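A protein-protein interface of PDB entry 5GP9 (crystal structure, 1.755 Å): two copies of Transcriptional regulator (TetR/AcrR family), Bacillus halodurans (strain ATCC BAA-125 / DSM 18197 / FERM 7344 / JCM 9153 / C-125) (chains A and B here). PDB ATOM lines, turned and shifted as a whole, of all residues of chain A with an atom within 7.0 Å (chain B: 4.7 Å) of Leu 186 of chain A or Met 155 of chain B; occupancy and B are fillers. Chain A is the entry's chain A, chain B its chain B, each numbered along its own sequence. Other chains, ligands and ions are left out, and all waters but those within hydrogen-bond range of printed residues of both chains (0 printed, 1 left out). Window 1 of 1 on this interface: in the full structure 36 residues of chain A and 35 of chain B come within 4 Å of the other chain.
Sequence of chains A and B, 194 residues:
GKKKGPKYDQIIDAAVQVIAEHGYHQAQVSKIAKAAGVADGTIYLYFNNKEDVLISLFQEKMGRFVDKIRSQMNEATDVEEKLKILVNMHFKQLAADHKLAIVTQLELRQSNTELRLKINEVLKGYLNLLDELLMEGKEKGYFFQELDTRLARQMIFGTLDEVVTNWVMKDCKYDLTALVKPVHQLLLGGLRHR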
ATOM      1  N   MET A 155     -24.494  17.374 -18.900  1.00  0.00           N
ATOM      2  CA  MET A 155     -23.786  18.685 -18.825  1.00  0.00           C
ATOM      3  C   MET A 155     -23.531  19.229 -20.240  1.00  0.00           C
ATOM      4  O   MET A 155     -23.729  20.404 -20.499  1.00  0.00           O
ATOM      5  CB  MET A 155     -22.467  18.501 -18.063  1.00  0.00           C
ATOM      6  CG  MET A 155     -21.725  19.842 -17.949  1.00  0.00           C
ATOM      7  SD  MET A 155     -20.101  19.908 -17.151  1.00  0.00           S
ATOM      8  CE  MET A 155     -19.445  19.000 -18.416  1.00  0.00           C
ATOM      9  N   GLY A 158     -27.022  19.892 -21.830  1.00  0.00           N
ATOM     10  CA  GLY A 158     -27.777  20.909 -21.158  1.00  0.00           C
ATOM     11  C   GLY A 158     -27.160  22.290 -21.370  1.00  0.00           C
ATOM     12  O   GLY A 158     -27.840  23.293 -21.479  1.00  0.00           O
ATOM     13  N   THR A 159     -25.841  22.290 -21.399  1.00  0.00           N
ATOM     14  CA  THR A 159     -25.096  23.537 -21.651  1.00  0.00           C
ATOM     15  C   THR A 159     -25.332  24.084 -23.043  1.00  0.00           C
ATOM     16  O   THR A 159     -25.662  25.301 -23.212  1.00  0.00           O
ATOM     17  CB  THR A 159     -23.573  23.383 -21.324  1.00  0.00           C
ATOM     18  OG1 THR A 159     -23.427  23.149 -19.941  1.00  0.00           O
ATOM     19  CG2 THR A 159     -22.888  24.699 -21.588  1.00  0.00           C
ATOM     20  N   LEU A 160     -25.107  23.278 -24.041  1.00  0.00           N
ATOM     21  CA  LEU A 160     -25.294  23.740 -25.453  1.00  0.00           C
ATOM     22  C   LEU A 160     -26.712  24.213 -25.717  1.00  0.00           C
ATOM     23  O   LEU A 160     -26.977  25.263 -26.247  1.00  0.00           O
ATOM     24  CB  LEU A 160     -24.938  22.641 -26.385  1.00  0.00           C
ATOM     25  CG  LEU A 160     -23.520  22.117 -26.426  1.00  0.00           C
ATOM     26  CD1 LEU A 160     -23.298  21.009 -27.454  1.00  0.00           C
ATOM     27  CD2 LEU A 160     -22.513  23.225 -26.644  1.00  0.00           C
ATOM     28  N   GLU A 162     -28.912  25.390 -23.489  1.00  0.00           N
ATOM     29  CA  GLU A 162     -29.129  26.593 -22.777  1.00  0.00           C
ATOM     30  C   GLU A 162     -28.509  27.806 -23.479  1.00  0.00           C
ATOM     31  O   GLU A 162     -29.144  28.844 -23.572  1.00  0.00           O
ATOM     32  CB  GLU A 162     -28.663  26.489 -21.351  1.00  0.00           C
ATOM     33  CG  GLU A 162     -28.887  27.685 -20.451  1.00  0.00           C
ATOM     34  CD  GLU A 162     -30.365  27.882 -20.039  1.00  0.00           C
ATOM     35  OE1 GLU A 162     -31.150  26.950 -20.217  1.00  0.00           O
ATOM     36  OE2 GLU A 162     -30.681  28.958 -19.576  1.00  0.00           O
ATOM     37  N   VAL A 163     -27.289  27.639 -23.992  1.00  0.00           N
ATOM     38  CA  VAL A 163     -26.630  28.731 -24.750  1.00  0.00           C
ATOM     39  C   VAL A 163     -27.507  29.071 -25.978  1.00  0.00           C
ATOM     40  O   VAL A 163     -27.859  30.217 -26.198  1.00  0.00           O
ATOM     41  CB  VAL A 163     -25.214  28.329 -25.125  1.00  0.00           C
ATOM     42  CG1 VAL A 163     -24.626  29.360 -26.155  1.00  0.00           C
ATOM     43  CG2 VAL A 163     -24.385  28.173 -23.891  1.00  0.00           C
ATOM     44  N   VAL A 180     -18.514  29.102 -29.943  1.00  0.00           N
ATOM     45  CA  VAL A 180     -18.008  27.756 -30.116  1.00  0.00           C
ATOM     46  C   VAL A 180     -16.773  27.532 -29.298  1.00  0.00           C
ATOM     47  O   VAL A 180     -16.724  26.602 -28.501  1.00  0.00           O
ATOM     48  CB  VAL A 180     -17.791  27.383 -31.620  1.00  0.00           C
ATOM     49  CG1 VAL A 180     -17.063  26.049 -31.796  1.00  0.00           C
ATOM     50  CG2 VAL A 180     -19.113  27.220 -32.367  1.00  0.00           C
ATOM     51  N   LYS A 181     -15.739  28.368 -29.481  1.00  0.00           N
ATOM     52  CA  LYS A 181     -14.502  28.119 -28.758  1.00  0.00           C
ATOM     53  C   LYS A 181     -14.682  28.257 -27.279  1.00  0.00           C
ATOM     54  O   LYS A 181     -14.265  27.352 -26.565  1.00  0.00           O
ATOM     55  CB  LYS A 181     -13.347  28.933 -29.325  1.00  0.00           C
ATOM     56  CG  LYS A 181     -12.066  28.883 -28.537  1.00  0.00           C
ATOM     57  CD  LYS A 181     -11.134  29.984 -29.048  1.00  0.00           C
ATOM     58  CE  LYS A 181      -9.857  30.132 -28.256  1.00  0.00           C
ATOM     59  NZ  LYS A 181      -8.827  29.208 -28.771  1.00  0.00           N
ATOM     60  N   PRO A 182     -15.269  29.365 -26.783  1.00  0.00           N
ATOM     61  CA  PRO A 182     -15.410  29.463 -25.333  1.00  0.00           C
ATOM     62  C   PRO A 182     -16.283  28.374 -24.676  1.00  0.00           C
ATOM     63  O   PRO A 182     -15.950  27.945 -23.576  1.00  0.00           O
ATOM     64  CB  PRO A 182     -15.973  30.857 -25.099  1.00  0.00           C
ATOM     65  CG  PRO A 182     -16.275  31.426 -26.383  1.00  0.00           C
ATOM     66  CD  PRO A 182     -15.662  30.617 -27.462  1.00  0.00           C
ATOM     67  N   VAL A 183     -17.303  27.892 -25.377  1.00  0.00           N
ATOM     68  CA  VAL A 183     -18.169  26.812 -24.759  1.00  0.00           C
ATOM     69  C   VAL A 183     -17.384  25.525 -24.679  1.00  0.00           C
ATOM     70  O   VAL A 183     -17.360  24.888 -23.677  1.00  0.00           O
ATOM     71  CB  VAL A 183     -19.478  26.626 -25.536  1.00  0.00           C
ATOM     72  CG1 VAL A 183     -20.181  25.365 -25.097  1.00  0.00           C
ATOM     73  CG2 VAL A 183     -20.381  27.843 -25.387  1.00  0.00           C
ATOM     74  N   HIS A 184     -16.695  25.201 -25.777  1.00  0.00           N
ATOM     75  CA  HIS A 184     -15.813  24.090 -25.842  1.00  0.00           C
ATOM     76  C   HIS A 184     -14.796  24.059 -24.694  1.00  0.00           C
ATOM     77  O   HIS A 184     -14.641  23.004 -24.030  1.00  0.00           O
ATOM     78  CB  HIS A 184     -15.074  24.149 -27.223  1.00  0.00           C
ATOM     79  CG  HIS A 184     -14.013  23.133 -27.377  1.00  0.00           C
ATOM     80  ND1 HIS A 184     -14.290  21.800 -27.514  1.00  0.00           N
ATOM     81  CD2 HIS A 184     -12.670  23.252 -27.406  1.00  0.00           C
ATOM     82  CE1 HIS A 184     -13.156  21.129 -27.623  1.00  0.00           C
ATOM     83  NE2 HIS A 184     -12.166  21.990 -27.560  1.00  0.00           N
ATOM     84  N   GLN A 185     -14.102  25.219 -24.479  1.00  0.00           N
ATOM     85  CA  GLN A 185     -13.112  25.269 -23.497  1.00  0.00           C
ATOM     86  C   GLN A 185     -13.681  25.109 -22.102  1.00  0.00           C
ATOM     87  O   GLN A 185     -13.099  24.468 -21.246  1.00  0.00           O
ATOM     88  CB  GLN A 185     -12.390  26.608 -23.551  1.00  0.00           C
ATOM     89  CG  GLN A 185     -11.835  27.039 -24.880  1.00  0.00           C
ATOM     90  CD  GLN A 185     -10.485  26.493 -25.240  1.00  0.00           C
ATOM     91  OE1 GLN A 185     -10.154  25.308 -25.035  1.00  0.00           O
ATOM     92  NE2 GLN A 185      -9.702  27.362 -25.876  1.00  0.00           N
ATOM     93  N   LEU A 186     -14.827  25.719 -21.891  1.00  0.00           N
ATOM     94  CA  LEU A 186     -15.486  25.731 -20.625  1.00  0.00           C
ATOM     95  C   LEU A 186     -15.950  24.324 -20.227  1.00  0.00           C
ATOM     96  O   LEU A 186     -15.777  23.922 -19.059  1.00  0.00           O
ATOM     97  CB  LEU A 186     -16.639  26.753 -20.628  1.00  0.00           C
ATOM     98  CG  LEU A 186     -17.478  26.893 -19.358  1.00  0.00           C
ATOM     99  CD1 LEU A 186     -16.699  27.357 -18.149  1.00  0.00           C
ATOM    100  CD2 LEU A 186     -18.661  27.864 -19.617  1.00  0.00           C
ATOM    101  N   LEU A 187     -16.489  23.559 -21.163  1.00  0.00           N
ATOM    102  CA  LEU A 187     -16.799  22.205 -20.942  1.00  0.00           C
ATOM    103  C   LEU A 187     -15.600  21.328 -20.587  1.00  0.00           C
ATOM    104  O   LEU A 187     -15.657  20.479 -19.713  1.00  0.00           O
ATOM    105  CB  LEU A 187     -17.584  21.601 -22.060  1.00  0.00           C
ATOM    106  CG  LEU A 187     -18.947  22.138 -22.455  1.00  0.00           C
ATOM    107  CD1 LEU A 187     -19.496  21.607 -23.779  1.00  0.00           C
ATOM    108  CD2 LEU A 187     -19.933  21.826 -21.338  1.00  0.00           C
ATOM    109  N   LEU A 188     -14.467  21.618 -21.179  1.00  0.00           N
ATOM    110  CA  LEU A 188     -13.225  20.905 -20.791  1.00  0.00           C
ATOM    111  C   LEU A 188     -12.642  21.287 -19.464  1.00  0.00           C
ATOM    112  O   LEU A 188     -12.084  20.432 -18.725  1.00  0.00           O
ATOM    113  CB  LEU A 188     -12.209  21.167 -21.906  1.00  0.00           C
ATOM    114  CG  LEU A 188     -12.612  20.574 -23.257  1.00  0.00           C
ATOM    115  CD1 LEU A 188     -11.667  21.039 -24.373  1.00  0.00           C
ATOM    116  CD2 LEU A 188     -12.614  19.067 -23.297  1.00  0.00           C
ATOM    117  N   GLY A 189     -12.640  22.569 -19.134  1.00  0.00           N
ATOM    118  CA  GLY A 189     -11.992  22.980 -17.892  1.00  0.00           C
ATOM    119  C   GLY A 189     -12.795  23.371 -16.707  1.00  0.00           C
ATOM    120  O   GLY A 189     -12.220  23.651 -15.637  1.00  0.00           O
ATOM    121  N   GLY A 190     -14.127  23.387 -16.854  1.00  0.00           N
ATOM    122  CA  GLY A 190     -14.972  23.823 -15.800  1.00  0.00           C
ATOM    123  C   GLY A 190     -14.744  25.211 -15.311  1.00  0.00           C
ATOM    124  O   GLY A 190     -14.190  26.116 -16.035  1.00  0.00           O
ATOM    125  N   LEU A 191     -15.165  25.449 -14.093  1.00  0.00           N
ATOM    126  CA  LEU A 191     -15.012  26.739 -13.508  1.00  0.00           C
ATOM    127  C   LEU A 191     -13.523  27.023 -13.145  1.00  0.00           C
ATOM    128  O   LEU A 191     -13.115  28.205 -13.130  1.00  0.00           O
ATOM    129  CB  LEU A 191     -15.865  26.924 -12.280  1.00  0.00           C
ATOM    130  CG  LEU A 191     -17.392  26.766 -12.561  1.00  0.00           C
ATOM    131  CD1 LEU A 191     -18.205  27.002 -11.334  1.00  0.00           C
ATOM    132  CD2 LEU A 191     -17.839  27.720 -13.643  1.00  0.00           C
ATOM    133  N   ARG A 192     -12.784  25.968 -12.805  1.00  0.00           N
ATOM    134  CA  ARG A 192     -11.429  26.126 -12.204  1.00  0.00           C
ATOM    135  C   ARG A 192     -10.305  26.480 -13.160  1.00  0.00           C
ATOM    136  O   ARG A 192      -9.383  27.230 -12.728  1.00  0.00           O
ATOM    137  CB  ARG A 192     -11.021  24.876 -11.467  1.00  0.00           C
ATOM    138  CG  ARG A 192     -11.680  24.653 -10.155  1.00  0.00           C
ATOM    139  CD  ARG A 192     -11.221  23.331  -9.616  1.00  0.00           C
ATOM    140  NE  ARG A 192     -11.799  22.973  -8.309  1.00  0.00           N
ATOM    141  CZ  ARG A 192     -12.071  21.713  -7.925  1.00  0.00           C
ATOM    142  NH1 ARG A 192     -11.830  20.662  -8.700  1.00  0.00           N
ATOM    143  NH2 ARG A 192     -12.549  21.491  -6.698  1.00  0.00           N
ATOM    144  N   HIS A 193     -10.375  25.958 -14.391  1.00  0.00           N
ATOM    145  CA  HIS A 193      -9.246  25.879 -15.325  1.00  0.00           C
ATOM    146  C   HIS A 193      -9.458  26.441 -16.699  1.00  0.00           C
ATOM    147  O   HIS A 193     -10.339  26.023 -17.445  1.00  0.00           O
ATOM    148  CB  HIS A 193      -8.920  24.395 -15.598  1.00  0.00           C
ATOM    149  CG  HIS A 193      -8.774  23.565 -14.370  1.00  0.00           C
ATOM    150  ND1 HIS A 193      -7.721  23.733 -13.493  1.00  0.00           N
ATOM    151  CD2 HIS A 193      -9.510  22.533 -13.886  1.00  0.00           C
ATOM    152  CE1 HIS A 193      -7.822  22.856 -12.510  1.00  0.00           C
ATOM    153  NE2 HIS A 193      -8.897  22.119 -12.719  1.00  0.00           N
ATOM    154  N   ARG A 194      -8.672  27.447 -17.009  1.00  0.00           N
ATOM    155  CA  ARG A 194      -8.310  27.877 -18.381  1.00  0.00           C
ATOM    156  C   ARG A 194      -7.959  29.337 -18.415  1.00  0.00           C
ATOM    157  O   ARG A 194      -7.444  29.795 -19.415  1.00  0.00           O
ATOM    158  CB  ARG A 194      -9.208  27.504 -19.553  1.00  0.00           C
ATOM    159  CG  ARG A 194      -8.899  26.184 -20.106  1.00  0.00           C
ATOM    160  CD  ARG A 194     -10.208  25.571 -20.657  1.00  0.00           C
ATOM    161  NE  ARG A 194      -9.987  24.227 -21.087  1.00  0.00           N
ATOM    162  CZ  ARG A 194      -9.252  23.874 -22.166  1.00  0.00           C
ATOM    163  NH1 ARG A 194      -9.024  22.565 -22.449  1.00  0.00           N
ATOM    164  NH2 ARG A 194      -8.746  24.813 -22.988  1.00  0.00           N
ATOM    165  N   LEU B 147     -12.749  33.802 -16.993  1.00  0.00           N
ATOM    166  CA  LEU B 147     -14.018  33.100 -17.068  1.00  0.00           C
ATOM    167  C   LEU B 147     -15.153  34.020 -17.472  1.00  0.00           C
ATOM    168  O   LEU B 147     -15.330  35.038 -16.894  1.00  0.00           O
ATOM    169  CB  LEU B 147     -14.341  32.465 -15.746  1.00  0.00           C
ATOM    170  CG  LEU B 147     -15.635  31.668 -15.631  1.00  0.00           C
ATOM    171  CD1 LEU B 147     -15.554  30.400 -16.414  1.00  0.00           C
ATOM    172  CD2 LEU B 147     -15.874  31.324 -14.196  1.00  0.00           C
ATOM    173  N   LEU B 151     -21.658  32.777 -19.695  1.00  0.00           N
ATOM    174  CA  LEU B 151     -21.569  31.405 -20.148  1.00  0.00           C
ATOM    175  C   LEU B 151     -21.512  30.408 -18.997  1.00  0.00           C
ATOM    176  O   LEU B 151     -22.102  29.367 -19.058  1.00  0.00           O
ATOM    177  CB  LEU B 151     -20.369  31.175 -21.049  1.00  0.00           C
ATOM    178  CG  LEU B 151     -20.401  31.670 -22.477  1.00  0.00           C
ATOM    179  CD1 LEU B 151     -19.096  31.391 -23.175  1.00  0.00           C
ATOM    180  CD2 LEU B 151     -21.534  31.033 -23.242  1.00  0.00           C
ATOM    181  N   ALA B 152     -20.776  30.757 -17.970  1.00  0.00           N
ATOM    182  CA  ALA B 152     -20.667  29.897 -16.830  1.00  0.00           C
ATOM    183  C   ALA B 152     -22.022  29.718 -16.128  1.00  0.00           C
ATOM    184  O   ALA B 152     -22.355  28.679 -15.711  1.00  0.00           O
ATOM    185  CB  ALA B 152     -19.629  30.398 -15.865  1.00  0.00           C
ATOM    186  N   ARG B 153     -22.756  30.791 -15.992  1.00  0.00           N
ATOM    187  CA  ARG B 153     -24.109  30.745 -15.460  1.00  0.00           C
ATOM    188  C   ARG B 153     -24.963  29.790 -16.256  1.00  0.00           C
ATOM    189  O   ARG B 153     -25.676  29.017 -15.720  1.00  0.00           O
ATOM    190  CB  ARG B 153     -24.717  32.146 -15.480  1.00  0.00           C
ATOM    191  CG  ARG B 153     -26.194  32.234 -15.215  1.00  0.00           C
ATOM    192  CD  ARG B 153     -26.854  33.186 -16.193  1.00  0.00           C
ATOM    193  NE  ARG B 153     -26.882  34.537 -15.690  1.00  0.00           N
ATOM    194  CZ  ARG B 153     -27.664  35.489 -16.158  1.00  0.00           C
ATOM    195  NH1 ARG B 153     -28.451  35.233 -17.163  1.00  0.00           N
ATOM    196  NH2 ARG B 153     -27.651  36.677 -15.616  1.00  0.00           N
ATOM    197  N   GLN B 154     -24.840  29.869 -17.561  1.00  0.00           N
ATOM    198  CA  GLN B 154     -25.612  29.033 -18.447  1.00  0.00           C
ATOM    199  C   GLN B 154     -25.184  27.566 -18.377  1.00  0.00           C
ATOM    200  O   GLN B 154     -25.991  26.709 -18.433  1.00  0.00           O
ATOM    201  CB  GLN B 154     -25.625  29.574 -19.884  1.00  0.00           C
ATOM    202  CG  GLN B 154     -26.211  30.961 -19.961  1.00  0.00           C
ATOM    203  CD  GLN B 154     -26.059  31.618 -21.306  1.00  0.00           C
ATOM    204  OE1 GLN B 154     -25.384  31.157 -22.168  1.00  0.00           O
ATOM    205  NE2 GLN B 154     -26.727  32.699 -21.462  1.00  0.00           N
ATOM    206  N   MET B 155     -23.890  27.326 -18.273  1.00  0.00           N
ATOM    207  CA  MET B 155     -23.407  25.985 -17.963  1.00  0.00           C
ATOM    208  C   MET B 155     -23.952  25.434 -16.618  1.00  0.00           C
ATOM    209  O   MET B 155     -24.509  24.331 -16.610  1.00  0.00           O
ATOM    210  CB  MET B 155     -21.901  25.896 -17.950  1.00  0.00           C
ATOM    211  CG  MET B 155     -21.453  24.463 -17.756  1.00  0.00           C
ATOM    212  SD  MET B 155     -19.612  24.374 -17.744  1.00  0.00           S
ATOM    213  CE  MET B 155     -19.277  25.244 -16.244  1.00  0.00           C
ATOM    214  N   ILE B 156     -23.875  26.197 -15.558  1.00  0.00           N
ATOM    215  CA  ILE B 156     -24.281  25.708 -14.242  1.00  0.00           C
ATOM    216  C   ILE B 156     -25.819  25.479 -14.281  1.00  0.00           C
ATOM    217  O   ILE B 156     -26.291  24.344 -14.059  1.00  0.00           O
ATOM    218  CB  ILE B 156     -23.931  26.620 -13.101  1.00  0.00           C
ATOM    219  CG1 ILE B 156     -22.397  26.758 -12.947  1.00  0.00           C
ATOM    220  CG2 ILE B 156     -24.642  26.197 -11.824  1.00  0.00           C
ATOM    221  CD1 ILE B 156     -21.968  27.924 -12.159  1.00  0.00           C
ATOM    222  N   PHE B 157     -26.563  26.484 -14.686  1.00  0.00           N
ATOM    223  CA  PHE B 157     -28.040  26.397 -14.562  1.00  0.00           C
ATOM    224  C   PHE B 157     -28.501  25.343 -15.585  1.00  0.00           C
ATOM    225  O   PHE B 157     -29.336  24.457 -15.291  1.00  0.00           O
ATOM    226  CB  PHE B 157     -28.729  27.691 -14.836  1.00  0.00           C
ATOM    227  CG  PHE B 157     -30.243  27.491 -14.930  1.00  0.00           C
ATOM    228  CD1 PHE B 157     -30.957  27.390 -13.713  1.00  0.00           C
ATOM    229  CD2 PHE B 157     -30.864  27.333 -16.155  1.00  0.00           C
ATOM    230  CE1 PHE B 157     -32.358  27.081 -13.730  1.00  0.00           C
ATOM    231  CE2 PHE B 157     -32.260  27.102 -16.152  1.00  0.00           C
ATOM    232  CZ  PHE B 157     -32.944  26.973 -14.975  1.00  0.00           C
ATOM    233  N   GLY B 158     -27.931  25.319 -16.806  1.00  0.00           N
ATOM    234  CA  GLY B 158     -28.330  24.418 -17.805  1.00  0.00           C
ATOM    235  C   GLY B 158     -28.032  22.959 -17.488  1.00  0.00           C
ATOM    236  O   GLY B 158     -28.848  22.053 -17.769  1.00  0.00           O
ATOM    237  N   THR B 159     -26.920  22.716 -16.782  1.00  0.00           N
ATOM    238  CA  THR B 159     -26.583  21.381 -16.382  1.00  0.00           C
ATOM    239  C   THR B 159     -27.529  20.941 -15.223  1.00  0.00           C
ATOM    240  O   THR B 159     -28.059  19.814 -15.291  1.00  0.00           O
ATOM    241  CB  THR B 159     -25.118  21.349 -15.899  1.00  0.00           C
ATOM    242  OG1 THR B 159     -24.303  21.567 -17.074  1.00  0.00           O
ATOM    243  CG2 THR B 159     -24.812  19.942 -15.349  1.00  0.00           C
ATOM    244  N   LEU B 187     -18.911  20.349 -12.590  1.00  0.00           N
ATOM    245  CA  LEU B 187     -18.973  21.754 -12.949  1.00  0.00           C
ATOM    246  C   LEU B 187     -17.598  22.471 -12.551  1.00  0.00           C
ATOM    247  O   LEU B 187     -17.102  23.363 -13.291  1.00  0.00           O
ATOM    248  CB  LEU B 187     -20.078  22.472 -12.258  1.00  0.00           C
ATOM    249  CG  LEU B 187     -21.497  22.036 -12.688  1.00  0.00           C
ATOM    250  CD1 LEU B 187     -22.480  22.614 -11.745  1.00  0.00           C
ATOM    251  CD2 LEU B 187     -21.723  22.540 -14.099  1.00  0.00           C
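Among the printed residues, pairs that only touch across the chains: Met 155 of chain A with Thr 159 of chain B, Thr 159 of chain A with Met 155 of chain B, Gly 190 of chain A with Leu 187 of chain B, Val 163 of chain A with Gln 154 of chain B, Glu 162 of chain A with Gln 154 of chain B, Leu 186 of chain A with Met 155 of chain B, Leu 186 of chain A with Leu 147 of chain B, Pro 182 of chain A with Leu 151 of chain B, Gly 158 of chain A with Gly 158 of chain B, Glu 162 of chain A with Phe 157 of chain B, Leu 186 of chain A with Leu 151 of chain B, Leu 191 of chain A with Met 155 of chain B, Leu 191 of chain A with Ala 152 of chain B, Leu 186 of chain A with Ala 152 of chain B and Leu 191 of chain A with Ile 156 of chain B.
OG1 of Thr 159 of chain B sits at hydrogen-bond distance from OG1 of Thr 159 of chain A, at 3.4 Å. The backbone NH of Leu 191 of chain A is in hydrogen-bond range of the backbone carbonyl oxygen of Leu 187 of chain B (3.0 Å).
The side-chain hydroxyl (OG1) of Thr 159 of chain A is in hydrogen-bond range of the backbone carbonyl oxygen (O) of Met 155 of chain A, 2.8 Å away. The backbone carbonyl oxygen (O) of Met 155 of chain B sits at hydrogen-bond distance from the side-chain hydroxyl (OG1) of Thr 159 of chain B, 2.8 Å away.
Hydrophobic or aromatic side chains of chain A that line the printed part of chain B: Met 155, Val 163, Pro 182, Leu 186 and Leu 191. Along chain A the printed residues that touch a printed residue of chain B span positions 155 to 191. Printed residues of chain B that touch a printed residue of chain A: Leu 147, Leu 151, Ala 152, Gln 154, Met 155, Ile 156, Phe 157, Gly 158, Thr 159 and Leu 187. Among the printed residues, 17 pairs touch across the chains. Among the printed residues, no Asp or Glu carboxylate lies within 4 Å of a Lys or Arg side-chain nitrogen of the other chain.
Of chain B, only Leu 147 (3.7 Å), Leu 151 (3.8 Å), Ala 152 (3.9 Å) and Met 155 (3.7 Å) come within 4 Å of Leu 186 of chain A. Printed residues of chain A within 4 Å of Phe 157 of chain B: Glu 162. Of the printed residues of chain A, Leu 187 of chain B touches Gly 190 (3.3 Å) and Leu 191 (3.0 Å). Of the printed residues of chain B, Leu 191 of chain A touches Ala 152 (3.9 Å), Met 155 (3.9 Å), Ile 156 (3.96 Å) and Leu 187 (3.0 Å). Leu 160 of chain A touches none of the printed residues of chain B. The nearest printed residue of chain B that does not touch Leu 186 of chain A is Leu 187 of chain B (5.9 Å). The nearest residue of chain A that does not touch Met 155 of chain B is Leu 187 of chain A (4.4 Å). The nearest printed residue of chain B that does not touch Gly 190 of chain A is Leu 147 of chain B (4.5 Å).
Met 155 of chain A touches Thr 159 of chain B, and with the chains exchanged Thr 159 of chain A touches Met 155 of chain B. Gly 158 of chain A touches its own counterpart, Gly 158 of chain B. Thr 159 of chain B touches its own counterpart, Thr 159 of chain A. 4 positions are printed for both chains. Of the 17 pairs that touch across the chains among the printed residues, 4 have their exchanged pair printed and touching as well.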
